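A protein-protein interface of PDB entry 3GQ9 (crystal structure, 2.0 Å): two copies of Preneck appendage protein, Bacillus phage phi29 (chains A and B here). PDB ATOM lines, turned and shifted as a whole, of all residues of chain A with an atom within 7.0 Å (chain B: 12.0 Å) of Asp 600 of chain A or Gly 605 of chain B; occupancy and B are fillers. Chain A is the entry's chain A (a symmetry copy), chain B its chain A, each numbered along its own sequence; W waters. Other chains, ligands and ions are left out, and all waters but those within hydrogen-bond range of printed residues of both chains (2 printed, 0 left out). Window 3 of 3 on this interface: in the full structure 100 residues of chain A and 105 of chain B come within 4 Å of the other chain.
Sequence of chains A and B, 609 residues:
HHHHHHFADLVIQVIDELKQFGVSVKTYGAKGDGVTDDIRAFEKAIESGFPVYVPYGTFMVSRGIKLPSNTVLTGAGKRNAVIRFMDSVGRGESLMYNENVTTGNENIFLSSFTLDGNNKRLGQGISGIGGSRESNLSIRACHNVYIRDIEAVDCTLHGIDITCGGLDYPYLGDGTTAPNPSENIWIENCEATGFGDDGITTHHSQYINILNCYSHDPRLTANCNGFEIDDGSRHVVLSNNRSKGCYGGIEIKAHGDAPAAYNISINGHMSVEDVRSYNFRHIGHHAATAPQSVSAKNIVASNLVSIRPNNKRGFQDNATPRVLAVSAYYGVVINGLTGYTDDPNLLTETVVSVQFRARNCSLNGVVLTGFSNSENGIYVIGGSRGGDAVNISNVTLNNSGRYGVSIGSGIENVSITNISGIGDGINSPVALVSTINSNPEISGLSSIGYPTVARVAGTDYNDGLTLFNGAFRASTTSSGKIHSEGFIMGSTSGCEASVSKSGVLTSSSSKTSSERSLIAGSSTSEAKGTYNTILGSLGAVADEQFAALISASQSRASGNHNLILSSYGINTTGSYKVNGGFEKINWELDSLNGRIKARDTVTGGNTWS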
ATOM      1  N   ASN A 586     -17.602 -25.009 -17.293  1.00  0.00           N
ATOM      2  CA  ASN A 586     -18.505 -24.798 -18.438  1.00  0.00           C
ATOM      3  C   ASN A 586     -19.936 -24.370 -18.112  1.00  0.00           C
ATOM      4  O   ASN A 586     -20.652 -23.912 -18.995  1.00  0.00           O
ATOM      5  CB  ASN A 586     -18.521 -26.041 -19.329  1.00  0.00           C
ATOM      6  CG  ASN A 586     -17.217 -26.216 -20.112  1.00  0.00           C
ATOM      7  OD1 ASN A 586     -16.812 -27.339 -20.444  1.00  0.00           O
ATOM      8  ND2 ASN A 586     -16.572 -25.110 -20.421  1.00  0.00           N
ATOM      9  N   LYS A 597     -25.212 -19.500 -15.668  1.00  0.00           N
ATOM     10  CA  LYS A 597     -24.168 -19.207 -16.658  1.00  0.00           C
ATOM     11  C   LYS A 597     -23.737 -20.442 -17.444  1.00  0.00           C
ATOM     12  O   LYS A 597     -23.473 -21.481 -16.853  1.00  0.00           O
ATOM     13  CB  LYS A 597     -22.943 -18.621 -15.950  1.00  0.00           C
ATOM     14  CG  LYS A 597     -23.159 -17.216 -15.357  1.00  0.00           C
ATOM     15  CD  LYS A 597     -21.915 -16.775 -14.580  1.00  0.00           C
ATOM     16  CE  LYS A 597     -21.952 -15.298 -14.224  1.00  0.00           C
ATOM     17  NZ  LYS A 597     -20.645 -14.900 -13.598  1.00  0.00           N
ATOM     18  N   ALA A 598     -23.691 -20.324 -18.772  1.00  0.00           N
ATOM     19  CA  ALA A 598     -23.054 -21.316 -19.631  1.00  0.00           C
ATOM     20  C   ALA A 598     -21.864 -20.673 -20.333  1.00  0.00           C
ATOM     21  O   ALA A 598     -21.901 -19.482 -20.660  1.00  0.00           O
ATOM     22  CB  ALA A 598     -24.028 -21.836 -20.674  1.00  0.00           C
ATOM     23  N   ARG A 599     -20.820 -21.460 -20.580  1.00  0.00           N
ATOM     24  CA  ARG A 599     -19.713 -20.994 -21.421  1.00  0.00           C
ATOM     25  C   ARG A 599     -20.194 -20.789 -22.866  1.00  0.00           C
ATOM     26  O   ARG A 599     -19.841 -19.789 -23.508  1.00  0.00           O
ATOM     27  CB  ARG A 599     -18.561 -22.001 -21.424  1.00  0.00           C
ATOM     28  CG  ARG A 599     -17.357 -21.511 -22.226  1.00  0.00           C
ATOM     29  CD  ARG A 599     -16.143 -22.408 -22.048  1.00  0.00           C
ATOM     30  NE  ARG A 599     -15.633 -22.365 -20.680  1.00  0.00           N
ATOM     31  CZ  ARG A 599     -14.773 -21.456 -20.215  1.00  0.00           C
ATOM     32  NH1 ARG A 599     -14.328 -20.492 -21.004  1.00  0.00           N
ATOM     33  NH2 ARG A 599     -14.366 -21.510 -18.955  1.00  0.00           N
ATOM     34  N   ASP A 600     -20.981 -21.746 -23.377  1.00  0.00           N
ATOM     35  CA  ASP A 600     -21.499 -21.650 -24.745  1.00  0.00           C
ATOM     36  C   ASP A 600     -22.908 -21.025 -24.745  1.00  0.00           C
ATOM     37  O   ASP A 600     -23.041 -19.826 -24.492  1.00  0.00           O
ATOM     38  CB  ASP A 600     -21.432 -23.008 -25.481  1.00  0.00           C
ATOM     39  CG  ASP A 600     -21.723 -22.889 -26.976  1.00  0.00           C
ATOM     40  OD1 ASP A 600     -21.361 -21.858 -27.597  1.00  0.00           O
ATOM     41  OD2 ASP A 600     -22.315 -23.836 -27.538  1.00  0.00           O
ATOM     42  N   THR A 601     -23.946 -21.818 -25.000  1.00  0.00           N
ATOM     43  CA  THR A 601     -25.294 -21.271 -25.122  1.00  0.00           C
ATOM     44  C   THR A 601     -26.246 -21.706 -24.014  1.00  0.00           C
ATOM     45  O   THR A 601     -26.056 -22.758 -23.398  1.00  0.00           O
ATOM     46  CB  THR A 601     -25.939 -21.712 -26.438  1.00  0.00           C
ATOM     47  OG1 THR A 601     -25.959 -23.148 -26.500  1.00  0.00           O
ATOM     48  CG2 THR A 601     -25.164 -21.142 -27.639  1.00  0.00           C
ATOM     49  N   VAL A 602     -27.241 -20.865 -23.742  1.00  0.00           N
ATOM     50  CA  VAL A 602     -28.399 -21.263 -22.944  1.00  0.00           C
ATOM     51  C   VAL A 602     -29.622 -21.136 -23.854  1.00  0.00           C
ATOM     52  O   VAL A 602     -29.858 -20.072 -24.431  1.00  0.00           O
ATOM     53  CB  VAL A 602     -28.603 -20.374 -21.693  1.00  0.00           C
ATOM     54  CG1 VAL A 602     -29.610 -21.014 -20.743  1.00  0.00           C
ATOM     55  CG2 VAL A 602     -27.292 -20.141 -20.972  1.00  0.00           C
ATOM     56  N   THR B 601     -30.057 -13.153 -13.968  1.00  0.00           N
ATOM     57  CA  THR B 601     -29.868 -13.388 -15.396  1.00  0.00           C
ATOM     58  C   THR B 601     -29.546 -14.833 -15.753  1.00  0.00           C
ATOM     59  O   THR B 601     -29.020 -15.583 -14.926  1.00  0.00           O
ATOM     60  CB  THR B 601     -28.711 -12.544 -15.934  1.00  0.00           C
ATOM     61  OG1 THR B 601     -27.515 -12.856 -15.200  1.00  0.00           O
ATOM     62  CG2 THR B 601     -29.030 -11.044 -15.812  1.00  0.00           C
ATOM     63  N   VAL B 602     -29.905 -15.222 -16.974  1.00  0.00           N
ATOM     64  CA  VAL B 602     -29.400 -16.454 -17.578  1.00  0.00           C
ATOM     65  C   VAL B 602     -28.614 -16.041 -18.822  1.00  0.00           C
ATOM     66  O   VAL B 602     -29.144 -15.339 -19.687  1.00  0.00           O
ATOM     67  CB  VAL B 602     -30.529 -17.430 -17.992  1.00  0.00           C
ATOM     68  CG1 VAL B 602     -29.953 -18.804 -18.314  1.00  0.00           C
ATOM     69  CG2 VAL B 602     -31.571 -17.551 -16.899  1.00  0.00           C
ATOM     70  N   THR B 603     -27.347 -16.455 -18.907  1.00  0.00           N
ATOM     71  CA  THR B 603     -26.474 -16.002 -20.000  1.00  0.00           C
ATOM     72  C   THR B 603     -25.538 -17.086 -20.512  1.00  0.00           C
ATOM     73  O   THR B 603     -25.120 -17.992 -19.759  1.00  0.00           O
ATOM     74  CB  THR B 603     -25.587 -14.802 -19.582  1.00  0.00           C
ATOM     75  OG1 THR B 603     -24.812 -15.158 -18.439  1.00  0.00           O
ATOM     76  CG2 THR B 603     -26.416 -13.561 -19.242  1.00  0.00           C
ATOM     77  N   GLY B 604     -25.201 -16.970 -21.795  1.00  0.00           N
ATOM     78  CA  GLY B 604     -24.186 -17.805 -22.422  1.00  0.00           C
ATOM     79  C   GLY B 604     -22.954 -16.945 -22.599  1.00  0.00           C
ATOM     80  O   GLY B 604     -22.940 -15.794 -22.171  1.00  0.00           O
ATOM     81  N   GLY B 605     -21.916 -17.498 -23.222  1.00  0.00           N
ATOM     82  CA  GLY B 605     -20.694 -16.740 -23.512  1.00  0.00           C
ATOM     83  C   GLY B 605     -19.865 -16.344 -22.301  1.00  0.00           C
ATOM     84  O   GLY B 605     -19.097 -15.371 -22.353  1.00  0.00           O
ATOM     85  N   ASN B 606     -19.988 -17.103 -21.214  1.00  0.00           N
ATOM     86  CA  ASN B 606     -19.276 -16.796 -19.982  1.00  0.00           C
ATOM     87  C   ASN B 606     -17.878 -17.384 -19.902  1.00  0.00           C
ATOM     88  O   ASN B 606     -17.592 -18.430 -20.492  1.00  0.00           O
ATOM     89  CB  ASN B 606     -20.089 -17.281 -18.777  1.00  0.00           C
ATOM     90  CG  ASN B 606     -21.322 -16.453 -18.554  1.00  0.00           C
ATOM     91  OD1 ASN B 606     -21.234 -15.349 -18.034  1.00  0.00           O
ATOM     92  ND2 ASN B 606     -22.477 -16.958 -18.987  1.00  0.00           N
ATOM     93  N   THR B 607     -17.008 -16.705 -19.161  1.00  0.00           N
ATOM     94  CA  THR B 607     -15.727 -17.276 -18.758  1.00  0.00           C
ATOM     95  C   THR B 607     -15.638 -17.192 -17.237  1.00  0.00           C
ATOM     96  O   THR B 607     -16.427 -16.499 -16.604  1.00  0.00           O
ATOM     97  CB  THR B 607     -14.519 -16.513 -19.354  1.00  0.00           C
ATOM     98  OG1 THR B 607     -14.563 -15.150 -18.913  1.00  0.00           O
ATOM     99  CG2 THR B 607     -14.541 -16.557 -20.872  1.00  0.00           C
ATOM    100  N   TRP B 608     -14.680 -17.900 -16.660  1.00  0.00           N
ATOM    101  CA  TRP B 608     -14.504 -17.905 -15.224  1.00  0.00           C
ATOM    102  C   TRP B 608     -13.156 -17.298 -14.826  1.00  0.00           C
ATOM    103  O   TRP B 608     -12.311 -17.964 -14.252  1.00  0.00           O
ATOM    104  CB  TRP B 608     -14.727 -19.316 -14.670  1.00  0.00           C
ATOM    105  CG  TRP B 608     -16.194 -19.600 -14.490  1.00  0.00           C
ATOM    106  CD1 TRP B 608     -16.911 -19.497 -13.326  1.00  0.00           C
ATOM    107  CD2 TRP B 608     -17.140 -19.971 -15.510  1.00  0.00           C
ATOM    108  NE1 TRP B 608     -18.235 -19.806 -13.555  1.00  0.00           N
ATOM    109  CE2 TRP B 608     -18.406 -20.096 -14.884  1.00  0.00           C
ATOM    110  CE3 TRP B 608     -17.040 -20.223 -16.884  1.00  0.00           C
ATOM    111  CZ2 TRP B 608     -19.567 -20.456 -15.591  1.00  0.00           C
ATOM    112  CZ3 TRP B 608     -18.189 -20.584 -17.585  1.00  0.00           C
ATOM    113  CH2 TRP B 608     -19.439 -20.701 -16.930  1.00  0.00           C
ATOM    114  N   SER B 609     -12.988 -16.012 -15.133  1.00  0.00           N
ATOM    115  CA  SER B 609     -11.718 -15.287 -14.910  1.00  0.00           C
ATOM    116  C   SER B 609     -11.917 -13.787 -14.702  1.00  0.00           C
ATOM    117  O   SER B 609     -12.773 -13.150 -15.341  1.00  0.00           O
ATOM    118  CB  SER B 609     -10.763 -15.485 -16.095  1.00  0.00           C
ATOM    119  OG  SER B 609     -11.447 -15.407 -17.342  1.00  0.00           O
ATOM    120  OXT SER B 609     -11.190 -13.178 -13.900  1.00  0.00           O
HETATM  121  O   HOH W   1     -17.310 -18.286 -23.321  1.00  0.00           O
HETATM  122  O   HOH W   2     -18.386 -16.531 -14.511  1.00  0.00           O
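Printed residues of chain B within 4 Å of Lys 597 of chain A: Thr 603 (3.5 Å), Asn 606 (3.5 Å) and Trp 608 (3.9 Å).
Ala 598 of chain A touches just these residues of chain B: Thr 603 (2.9 Å), Gly 604 (3.3 Å), Gly 605 (3.2 Å) and Asn 606 (3.1 Å).
Asp 600 of chain A touches just these residues of chain B: Gly 604 (3.1 Å) and Gly 605 (2.9 Å).
No residue of chain B comes within 4 Å of Thr 601 of chain A.
Of the printed residues of chain B, Val 602 of chain A touches Val 602 (3.3 Å), Thr 603 (3.3 Å) and Gly 604 (3.9 Å).
Of the printed residues of chain A, Thr 603 of chain B touches Lys 597 (3.5 Å), Ala 598 (2.9 Å) and Val 602 (3.3 Å).
Of the printed residues of chain A, Gly 604 of chain B touches Ala 598 (3.3 Å), Asp 600 (3.1 Å) and Val 602 (3.9 Å).
Of chain A, only Ala 598 (3.2 Å), Arg 599 (3.1 Å) and Asp 600 (2.9 Å) come within 4 Å of Gly 605 of chain B.
Of the printed residues of chain A, Trp 608 of chain B touches Asn 586 (3.9 Å), Lys 597 (3.9 Å) and Arg 599 (3.6 Å).
The nearest residue of chain B that does not touch Asp 600 of chain A is Asn 606 of chain B (5.2 Å).
The nearest printed residue of chain A that does not touch Gly 604 of chain B is Arg 599 of chain A (4.3 Å).
O of Arg 599 of chain A sits at hydrogen-bond distance from N of Gly 605 of chain B (3.1 Å).
N of Gly 605 of chain B is in hydrogen-bond range of O of Asp 600 of chain A (2.9 Å).
The backbone carbonyl oxygen (O) of Thr 603 of chain B is in hydrogen-bond range of the backbone NH (N) of Ala 598 of chain A (2.9 Å).
The backbone NH of Gly 605 of chain B lies within hydrogen-bond range of the backbone carbonyl oxygen of Ala 598 of chain A, at 3.2 Å.
ND2 of Asn 606 of chain B is in hydrogen-bond range of O of Ala 598 of chain A (3.1 Å).
Water W1 bridges the backbone carbonyl oxygen (O) of Asn 606 of chain B (2.8 Å) and the backbone carbonyl oxygen (O) of Arg 599 of chain A (2.9 Å).
Water W2 lies within hydrogen-bond range of the backbone carbonyl oxygen of Thr 607 of chain B (2.9 Å), the side-chain amino group of Lys 597 of chain A (2.9 Å) and the indole nitrogen of Trp 608 of chain B (3.4 Å).
Val 602 of chain A touches its own counterpart, Val 602 of chain B.
2 positions are printed for both chains.
Of the 17 pairs that touch across the chains among the printed residues, 1 has its exchanged pair printed and touching as well.
Of the 9 printed residues of chain B, 7 touch a printed residue of chain A.
Printed residues of chain B that touch a printed residue of chain A: Val 602, Thr 603, Gly 604, Gly 605, Asn 606, Thr 607 and Trp 608.
Hydrophobic or aromatic side chains of chain B that line the printed part of chain A: Val 602 and Trp 608.
Hydrophobic or aromatic side chains of chain A that line the printed part of chain B: Val 602.
Along chain A the printed residues that touch a printed residue of chain B span positions 586 to 602.
Among the printed residues, 17 pairs touch across the chains.
O of Thr 603 of chain B is in hydrogen-bond range of ND2 of Asn 606 of chain B (2.9 Å).
OG1 of Thr 607 of chain B sits at hydrogen-bond distance from OG of Ser 609 of chain B, at 3.5 Å.
NE of Arg 599 of chain A sits close to ND2 of Asn 586 of chain A, 2.9 Å away.
The side-chain amide nitrogen of Asn 606 of chain B sits at hydrogen-bond distance from the backbone carbonyl oxygen of Gly 604 of chain B (3.4 Å).
Among the printed residues, merely in contact across the chains: Asn 586 of chain A with Trp 608 of chain B, Lys 597 of chain A with Thr 603 of chain B, Lys 597 of chain A with Asn 606 of chain B, Lys 597 of chain A with Trp 608 of chain B, Ala 598 of chain A with Gly 604 of chain B, Arg 599 of chain A with Asn 606 of chain B, Arg 599 of chain A with Thr 607 of chain B, Arg 599 of chain A with Trp 608 of chain B, Asp 600 of chain A with Gly 604 of chain B, Val 602 of chain A with Val 602 of chain B, Val 602 of chain A with Thr 603 of chain B and Val 602 of chain A with Gly 604 of chain B.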
